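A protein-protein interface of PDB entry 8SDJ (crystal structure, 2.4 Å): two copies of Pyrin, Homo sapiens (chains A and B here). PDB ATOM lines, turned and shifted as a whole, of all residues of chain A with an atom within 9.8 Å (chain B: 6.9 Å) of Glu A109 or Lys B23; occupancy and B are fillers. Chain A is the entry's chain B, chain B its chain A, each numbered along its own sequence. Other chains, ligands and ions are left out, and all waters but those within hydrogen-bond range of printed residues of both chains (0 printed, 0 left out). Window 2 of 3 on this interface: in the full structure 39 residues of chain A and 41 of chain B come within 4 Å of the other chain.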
ATOM      1  N   ILE A  98     -15.773 -21.622  -4.573  1.00  0.00           N
ATOM      2  CA  ILE A  98     -15.044 -20.849  -3.585  1.00  0.00           C
ATOM      3  C   ILE A  98     -15.875 -20.716  -2.316  1.00  0.00           C
ATOM      4  O   ILE A  98     -15.382 -21.003  -1.233  1.00  0.00           O
ATOM      5  CB  ILE A  98     -14.628 -19.456  -4.111  1.00  0.00           C
ATOM      6  CG1 ILE A  98     -13.394 -19.512  -5.012  1.00  0.00           C
ATOM      7  CG2 ILE A  98     -14.421 -18.479  -2.967  1.00  0.00           C
ATOM      8  CD1 ILE A  98     -13.011 -18.163  -5.588  1.00  0.00           C
ATOM      9  N   LEU A 101     -15.726 -23.675  -0.392  1.00  0.00           N
ATOM     10  CA  LEU A 101     -14.442 -23.938   0.248  1.00  0.00           C
ATOM     11  C   LEU A 101     -14.358 -23.139   1.551  1.00  0.00           C
ATOM     12  O   LEU A 101     -13.768 -23.616   2.518  1.00  0.00           O
ATOM     13  CB  LEU A 101     -13.294 -23.619  -0.718  1.00  0.00           C
ATOM     14  CG  LEU A 101     -12.997 -24.721  -1.730  1.00  0.00           C
ATOM     15  CD1 LEU A 101     -12.373 -24.154  -3.004  1.00  0.00           C
ATOM     16  CD2 LEU A 101     -12.103 -25.786  -1.119  1.00  0.00           C
ATOM     17  N   ASP A 102     -14.987 -21.953   1.574  1.00  0.00           N
ATOM     18  CA  ASP A 102     -15.049 -21.090   2.742  1.00  0.00           C
ATOM     19  C   ASP A 102     -15.899 -21.752   3.817  1.00  0.00           C
ATOM     20  O   ASP A 102     -15.540 -21.704   4.994  1.00  0.00           O
ATOM     21  CB  ASP A 102     -15.591 -19.701   2.405  1.00  0.00           C
ATOM     22  CG  ASP A 102     -14.548 -18.868   1.689  1.00  0.00           C
ATOM     23  OD1 ASP A 102     -13.432 -19.416   1.447  1.00  0.00           O
ATOM     24  OD2 ASP A 102     -14.855 -17.695   1.373  1.00  0.00           O
ATOM     25  N   ALA A 103     -17.018 -22.349   3.375  1.00  0.00           N
ATOM     26  CA  ALA A 103     -17.859 -23.204   4.190  1.00  0.00           C
ATOM     27  C   ALA A 103     -16.965 -24.183   4.931  1.00  0.00           C
ATOM     28  O   ALA A 103     -17.056 -24.294   6.144  1.00  0.00           O
ATOM     29  CB  ALA A 103     -18.834 -23.956   3.314  1.00  0.00           C
ATOM     30  N   LEU A 104     -16.109 -24.886   4.183  1.00  0.00           N
ATOM     31  CA  LEU A 104     -15.194 -25.848   4.766  1.00  0.00           C
ATOM     32  C   LEU A 104     -14.071 -25.173   5.574  1.00  0.00           C
ATOM     33  O   LEU A 104     -13.603 -25.737   6.569  1.00  0.00           O
ATOM     34  CB  LEU A 104     -14.649 -26.739   3.648  1.00  0.00           C
ATOM     35  CG  LEU A 104     -15.682 -27.616   2.961  1.00  0.00           C
ATOM     36  CD1 LEU A 104     -15.014 -28.487   1.907  1.00  0.00           C
ATOM     37  CD2 LEU A 104     -16.416 -28.488   3.976  1.00  0.00           C
ATOM     38  N   ILE A 105     -13.628 -23.972   5.164  1.00  0.00           N
ATOM     39  CA  ILE A 105     -12.571 -23.273   5.898  1.00  0.00           C
ATOM     40  C   ILE A 105     -13.051 -22.860   7.299  1.00  0.00           C
ATOM     41  O   ILE A 105     -12.412 -23.166   8.293  1.00  0.00           O
ATOM     42  CB  ILE A 105     -11.995 -22.050   5.140  1.00  0.00           C
ATOM     43  CG1 ILE A 105     -11.183 -22.390   3.880  1.00  0.00           C
ATOM     44  CG2 ILE A 105     -11.222 -21.141   6.094  1.00  0.00           C
ATOM     45  CD1 ILE A 105     -10.387 -23.655   3.963  1.00  0.00           C
ATOM     46  N   GLY A 106     -14.097 -22.040   7.371  1.00  0.00           N
ATOM     47  CA  GLY A 106     -14.539 -21.507   8.646  1.00  0.00           C
ATOM     48  C   GLY A 106     -14.810 -22.625   9.652  1.00  0.00           C
ATOM     49  O   GLY A 106     -14.634 -22.428  10.851  1.00  0.00           O
ATOM     50  N   GLU A 107     -15.197 -23.800   9.137  1.00  0.00           N
ATOM     51  CA  GLU A 107     -15.566 -24.970   9.919  1.00  0.00           C
ATOM     52  C   GLU A 107     -14.426 -25.436  10.821  1.00  0.00           C
ATOM     53  O   GLU A 107     -14.594 -25.563  12.037  1.00  0.00           O
ATOM     54  CB  GLU A 107     -15.856 -26.140   8.981  1.00  0.00           C
ATOM     55  CG  GLU A 107     -16.799 -27.161   9.571  1.00  0.00           C
ATOM     56  CD  GLU A 107     -16.865 -28.455   8.780  1.00  0.00           C
ATOM     57  OE1 GLU A 107     -15.864 -29.199   8.803  1.00  0.00           O
ATOM     58  OE2 GLU A 107     -17.913 -28.711   8.142  1.00  0.00           O
ATOM     59  N   LEU A 108     -13.302 -25.790  10.187  1.00  0.00           N
ATOM     60  CA  LEU A 108     -12.104 -26.225  10.884  1.00  0.00           C
ATOM     61  C   LEU A 108     -11.541 -25.034  11.653  1.00  0.00           C
ATOM     62  O   LEU A 108     -11.275 -25.142  12.838  1.00  0.00           O
ATOM     63  CB  LEU A 108     -11.083 -26.770   9.876  1.00  0.00           C
ATOM     64  CG  LEU A 108     -11.501 -27.997   9.061  1.00  0.00           C
ATOM     65  CD1 LEU A 108     -10.362 -28.476   8.161  1.00  0.00           C
ATOM     66  CD2 LEU A 108     -11.980 -29.133   9.964  1.00  0.00           C
ATOM     67  N   GLU A 109     -11.463 -23.876  11.000  1.00  0.00           N
ATOM     68  CA  GLU A 109     -10.829 -22.712  11.592  1.00  0.00           C
ATOM     69  C   GLU A 109     -11.526 -22.290  12.877  1.00  0.00           C
ATOM     70  O   GLU A 109     -10.881 -21.700  13.740  1.00  0.00           O
ATOM     71  CB  GLU A 109     -10.684 -21.565  10.592  1.00  0.00           C
ATOM     72  CG  GLU A 109      -9.680 -21.902   9.500  1.00  0.00           C
ATOM     73  CD  GLU A 109      -8.805 -20.763   9.011  1.00  0.00           C
ATOM     74  OE1 GLU A 109      -9.362 -19.691   8.694  1.00  0.00           O
ATOM     75  OE2 GLU A 109      -7.567 -20.954   8.956  1.00  0.00           O
ATOM     76  N   ALA A 110     -12.815 -22.635  13.015  1.00  0.00           N
ATOM     77  CA  ALA A 110     -13.634 -22.159  14.124  1.00  0.00           C
ATOM     78  C   ALA A 110     -13.684 -23.160  15.281  1.00  0.00           C
ATOM     79  O   ALA A 110     -13.869 -22.771  16.439  1.00  0.00           O
ATOM     80  CB  ALA A 110     -15.016 -21.788  13.642  1.00  0.00           C
ATOM     81  N   LYS A 111     -13.533 -24.451  14.966  1.00  0.00           N
ATOM     82  CA  LYS A 111     -13.436 -25.452  16.014  1.00  0.00           C
ATOM     83  C   LYS A 111     -12.012 -25.461  16.575  1.00  0.00           C
ATOM     84  O   LYS A 111     -11.828 -25.564  17.784  1.00  0.00           O
ATOM     85  CB  LYS A 111     -13.962 -26.805  15.533  1.00  0.00           C
ATOM     86  CG  LYS A 111     -15.042 -27.403  16.424  1.00  0.00           C
ATOM     87  CD  LYS A 111     -14.477 -28.304  17.503  1.00  0.00           C
ATOM     88  CE  LYS A 111     -14.134 -29.692  16.993  1.00  0.00           C
ATOM     89  NZ  LYS A 111     -13.840 -30.619  18.111  1.00  0.00           N
ATOM     90  N   GLU A 112     -11.013 -25.314  15.695  1.00  0.00           N
ATOM     91  CA  GLU A 112      -9.631 -25.172  16.126  1.00  0.00           C
ATOM     92  C   GLU A 112      -9.445 -23.782  16.753  1.00  0.00           C
ATOM     93  O   GLU A 112      -9.171 -23.734  17.967  1.00  0.00           O
ATOM     94  CB  GLU A 112      -8.669 -25.369  14.953  1.00  0.00           C
ATOM     95  CG  GLU A 112      -8.302 -24.071  14.248  1.00  0.00           C
ATOM     96  CD  GLU A 112      -7.035 -24.143  13.409  1.00  0.00           C
ATOM     97  OE1 GLU A 112      -6.563 -25.270  13.114  1.00  0.00           O
ATOM     98  OE2 GLU A 112      -6.521 -23.069  13.045  1.00  0.00           O
ATOM     99  N   GLN B  18      -4.963 -30.513   5.917  1.00  0.00           N
ATOM    100  CA  GLN B  18      -6.254 -30.416   5.262  1.00  0.00           C
ATOM    101  C   GLN B  18      -6.609 -28.957   5.021  1.00  0.00           C
ATOM    102  O   GLN B  18      -6.989 -28.572   3.908  1.00  0.00           O
ATOM    103  CB  GLN B  18      -7.336 -31.121   6.080  1.00  0.00           C
ATOM    104  CG  GLN B  18      -7.288 -32.635   5.886  1.00  0.00           C
ATOM    105  CD  GLN B  18      -8.001 -33.454   6.939  1.00  0.00           C
ATOM    106  OE1 GLN B  18      -8.851 -32.960   7.684  1.00  0.00           O
ATOM    107  NE2 GLN B  18      -7.657 -34.732   7.003  1.00  0.00           N
ATOM    108  N   LEU B  19      -6.511 -28.155   6.081  1.00  0.00           N
ATOM    109  CA  LEU B  19      -6.794 -26.722   6.018  1.00  0.00           C
ATOM    110  C   LEU B  19      -5.766 -26.021   5.111  1.00  0.00           C
ATOM    111  O   LEU B  19      -5.958 -24.860   4.737  1.00  0.00           O
ATOM    112  CB  LEU B  19      -6.802 -26.198   7.464  1.00  0.00           C
ATOM    113  CG  LEU B  19      -7.138 -24.732   7.744  1.00  0.00           C
ATOM    114  CD1 LEU B  19      -8.480 -24.344   7.132  1.00  0.00           C
ATOM    115  CD2 LEU B  19      -7.121 -24.484   9.263  1.00  0.00           C
ATOM    116  N   GLU B  20      -4.679 -26.741   4.772  1.00  0.00           N
ATOM    117  CA  GLU B  20      -3.624 -26.241   3.908  1.00  0.00           C
ATOM    118  C   GLU B  20      -4.070 -26.438   2.463  1.00  0.00           C
ATOM    119  O   GLU B  20      -4.107 -25.471   1.706  1.00  0.00           O
ATOM    120  CB  GLU B  20      -2.274 -26.944   4.169  1.00  0.00           C
ATOM    121  CG  GLU B  20      -1.180 -25.999   4.633  1.00  0.00           C
ATOM    122  CD  GLU B  20       0.002 -26.510   5.428  1.00  0.00           C
ATOM    123  OE1 GLU B  20       0.308 -27.726   5.354  1.00  0.00           O
ATOM    124  OE2 GLU B  20       0.567 -25.684   6.150  1.00  0.00           O
ATOM    125  N   HIS B  21      -4.408 -27.687   2.105  1.00  0.00           N
ATOM    126  CA  HIS B  21      -4.901 -27.998   0.781  1.00  0.00           C
ATOM    127  C   HIS B  21      -6.164 -27.195   0.450  1.00  0.00           C
ATOM    128  O   HIS B  21      -6.301 -26.742  -0.682  1.00  0.00           O
ATOM    129  CB  HIS B  21      -5.094 -29.509   0.600  1.00  0.00           C
ATOM    130  CG  HIS B  21      -3.839 -30.297   0.702  1.00  0.00           C
ATOM    131  ND1 HIS B  21      -3.843 -31.664   0.895  1.00  0.00           N
ATOM    132  CD2 HIS B  21      -2.548 -29.923   0.677  1.00  0.00           C
ATOM    133  CE1 HIS B  21      -2.603 -32.099   0.967  1.00  0.00           C
ATOM    134  NE2 HIS B  21      -1.797 -31.059   0.827  1.00  0.00           N
ATOM    135  N   LEU B  22      -7.073 -27.063   1.411  1.00  0.00           N
ATOM    136  CA  LEU B  22      -8.332 -26.340   1.251  1.00  0.00           C
ATOM    137  C   LEU B  22      -8.196 -24.826   1.060  1.00  0.00           C
ATOM    138  O   LEU B  22      -9.206 -24.182   0.776  1.00  0.00           O
ATOM    139  CB  LEU B  22      -9.234 -26.545   2.476  1.00  0.00           C
ATOM    140  CG  LEU B  22      -9.897 -27.898   2.680  1.00  0.00           C
ATOM    141  CD1 LEU B  22     -10.867 -27.760   3.834  1.00  0.00           C
ATOM    142  CD2 LEU B  22     -10.607 -28.372   1.419  1.00  0.00           C
ATOM    143  N   LYS B  23      -7.022 -24.241   1.343  1.00  0.00           N
ATOM    144  CA  LYS B  23      -6.843 -22.798   1.292  1.00  0.00           C
ATOM    145  C   LYS B  23      -6.100 -22.437   0.006  1.00  0.00           C
ATOM    146  O   LYS B  23      -6.436 -21.429  -0.625  1.00  0.00           O
ATOM    147  CB  LYS B  23      -6.121 -22.306   2.548  1.00  0.00           C
ATOM    148  CG  LYS B  23      -7.012 -21.842   3.692  1.00  0.00           C
ATOM    149  CD  LYS B  23      -6.158 -21.267   4.810  1.00  0.00           C
ATOM    150  CE  LYS B  23      -6.953 -20.623   5.927  1.00  0.00           C
ATOM    151  NZ  LYS B  23      -6.075 -20.298   7.072  1.00  0.00           N
ATOM    152  N   LYS B  24      -5.140 -23.293  -0.404  1.00  0.00           N
ATOM    153  CA  LYS B  24      -4.601 -23.280  -1.764  1.00  0.00           C
ATOM    154  C   LYS B  24      -5.763 -23.354  -2.761  1.00  0.00           C
ATOM    155  O   LYS B  24      -5.942 -22.464  -3.585  1.00  0.00           O
ATOM    156  CB  LYS B  24      -3.532 -24.367  -1.934  1.00  0.00           C
ATOM    157  CG  LYS B  24      -2.545 -24.415  -0.770  1.00  0.00           C
ATOM    158  CD  LYS B  24      -1.210 -25.119  -0.964  1.00  0.00           C
ATOM    159  CE  LYS B  24      -0.261 -24.465  -1.945  1.00  0.00           C
ATOM    160  NZ  LYS B  24       0.505 -25.509  -2.677  1.00  0.00           N
ATOM    161  N   LEU B  25      -6.599 -24.388  -2.630  1.00  0.00           N
ATOM    162  CA  LEU B  25      -7.710 -24.572  -3.537  1.00  0.00           C
ATOM    163  C   LEU B  25      -8.499 -23.283  -3.605  1.00  0.00           C
ATOM    164  O   LEU B  25      -8.942 -22.908  -4.677  1.00  0.00           O
ATOM    165  CB  LEU B  25      -8.597 -25.714  -3.043  1.00  0.00           C
ATOM    166  CG  LEU B  25      -8.151 -27.086  -3.518  1.00  0.00           C
ATOM    167  CD1 LEU B  25      -9.008 -28.166  -2.874  1.00  0.00           C
ATOM    168  CD2 LEU B  25      -8.253 -27.149  -5.027  1.00  0.00           C
ATOM    169  N   ARG B  26      -8.638 -22.600  -2.470  1.00  0.00           N
ATOM    170  CA  ARG B  26      -9.428 -21.372  -2.443  1.00  0.00           C
ATOM    171  C   ARG B  26      -8.642 -20.225  -3.077  1.00  0.00           C
ATOM    172  O   ARG B  26      -9.214 -19.343  -3.722  1.00  0.00           O
ATOM    173  CB  ARG B  26      -9.834 -20.958  -1.031  1.00  0.00           C
ATOM    174  CG  ARG B  26     -10.782 -19.776  -1.009  1.00  0.00           C
ATOM    175  CD  ARG B  26     -10.513 -18.794   0.100  1.00  0.00           C
ATOM    176  NE  ARG B  26     -11.704 -17.973   0.285  1.00  0.00           N
ATOM    177  CZ  ARG B  26     -12.033 -16.897  -0.438  1.00  0.00           C
ATOM    178  NH1 ARG B  26     -13.147 -16.230  -0.174  1.00  0.00           N
ATOM    179  NH2 ARG B  26     -11.253 -16.484  -1.421  1.00  0.00           N
ATOM    180  N   LYS B  27      -7.317 -20.240  -2.919  1.00  0.00           N
ATOM    181  CA  LYS B  27      -6.564 -19.225  -3.623  1.00  0.00           C
ATOM    182  C   LYS B  27      -6.696 -19.513  -5.113  1.00  0.00           C
ATOM    183  O   LYS B  27      -7.023 -18.600  -5.871  1.00  0.00           O
ATOM    184  CB  LYS B  27      -5.144 -19.032  -3.073  1.00  0.00           C
ATOM    185  CG  LYS B  27      -4.401 -17.858  -3.705  1.00  0.00           C
ATOM    186  CD  LYS B  27      -3.872 -16.830  -2.715  1.00  0.00           C
ATOM    187  CE  LYS B  27      -2.803 -15.924  -3.294  1.00  0.00           C
ATOM    188  NZ  LYS B  27      -1.555 -16.656  -3.625  1.00  0.00           N
ATOM    189  N   SER B  28      -6.482 -20.783  -5.499  1.00  0.00           N
ATOM    190  CA  SER B  28      -6.575 -21.229  -6.885  1.00  0.00           C
ATOM    191  C   SER B  28      -7.902 -20.778  -7.491  1.00  0.00           C
ATOM    192  O   SER B  28      -7.977 -20.396  -8.646  1.00  0.00           O
ATOM    193  CB  SER B  28      -6.379 -22.699  -6.991  1.00  0.00           C
ATOM    194  OG  SER B  28      -6.408 -23.106  -8.363  1.00  0.00           O
ATOM    195  N   GLY B  29      -8.932 -20.725  -6.655  1.00  0.00           N
ATOM    196  CA  GLY B  29     -10.234 -20.268  -7.084  1.00  0.00           C
ATOM    197  C   GLY B  29     -10.184 -18.814  -7.534  1.00  0.00           C
ATOM    198  O   GLY B  29     -10.534 -18.540  -8.671  1.00  0.00           O
ATOM    199  N   GLU B  30      -9.734 -17.893  -6.664  1.00  0.00           N
ATOM    200  CA  GLU B  30      -9.801 -16.462  -6.963  1.00  0.00           C
ATOM    201  C   GLU B  30      -8.798 -16.052  -8.055  1.00  0.00           C
ATOM    202  O   GLU B  30      -9.083 -15.144  -8.841  1.00  0.00           O
ATOM    203  CB  GLU B  30      -9.706 -15.636  -5.684  1.00  0.00           C
ATOM    204  CG  GLU B  30      -8.940 -16.345  -4.590  1.00  0.00           C
ATOM    205  CD  GLU B  30      -8.742 -15.543  -3.323  1.00  0.00           C
ATOM    206  OE1 GLU B  30      -8.581 -14.312  -3.441  1.00  0.00           O
ATOM    207  OE2 GLU B  30      -8.750 -16.151  -2.229  1.00  0.00           O
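The side-chain carboxylate (OE2) of Glu A109 is in salt-bridge range of the side-chain amino group (NZ) of Lys B23 (2.5 Å).
The guanidinium group (NE) of Arg B26 is in salt-bridge range of the side-chain carboxylate (OD1) of Asp A102 (2.5 Å).
The guanidinium group (NH2) of Arg B26 lies within salt-bridge range of the side-chain carboxylate (OE2) of Glu B30, 2.7 Å away.
Arg B26 touches Ile A98.
C of Gly B29 touches CD1 of Ile A98 (3.5 Å).
Ile A98 touches Glu B30.
CD2 of Leu A101 touches O of Leu B22, 3.8 Å away.
Leu A101 touches Leu B25.
Leu A104 touches Leu B22.
Ile A105 touches Leu B22.
Lys B23 touches Ile A105.
OE2 of Glu A109 touches CD2 of Leu B19, at 3.6 Å.
OE1 of Glu A112 touches CD2 of Leu B19, 3.97 Å away.
Glu A109 touches just these residues of chain B: Leu B19 and Lys B23.
Lys B23 touches just these residues of chain A: Ile A105 (3.8 Å) and Glu A109 (2.5 Å).
Printed residues of chain A within 4 Å of Leu B19: Ile A105 (3.8 Å), Glu A109 (3.6 Å) and Glu A112 (3.97 Å).
Of the printed residues of chain B, Leu A101 touches Leu B22 and Leu B25.
Of the printed residues of chain A, Arg B26 touches Ile A98 (3.8 Å) and Asp A102 (2.5 Å).
Of the printed residues of chain B, Asp A102 touches Arg B26.
The nearest printed residue of chain B that does not touch Glu A109 is Glu B20 (7.7 Å).
The nearest residue of chain A that does not touch Lys B23 is Leu A101 (5.9 Å).
The nearest printed residue of chain A that does not touch Gly B29 is Leu A101 (6.0 Å).
Of the 13 printed residues of chain A, 7 touch a printed residue of chain B.
Printed residues of chain A that touch a printed residue of chain B: Ile A98, Leu A101, Asp A102, Leu A104, Ile A105, Glu A109 and Glu A112.
Hydrophobic or aromatic side chains of chain A within 4 Å of the printed part of chain B: Ile A98, Leu A101, Leu A104 and Ile A105.
Among the printed residues, Asp or Glu carboxylates within 4 Å of a Lys or Arg side-chain nitrogen of the other chain: Asp A102 with Arg B26 and Glu A109 with Lys B23.
No position is printed for both chains.
Of the 13 pairs that touch across the chains among the printed residues, none has its exchanged pair printed and touching as well.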
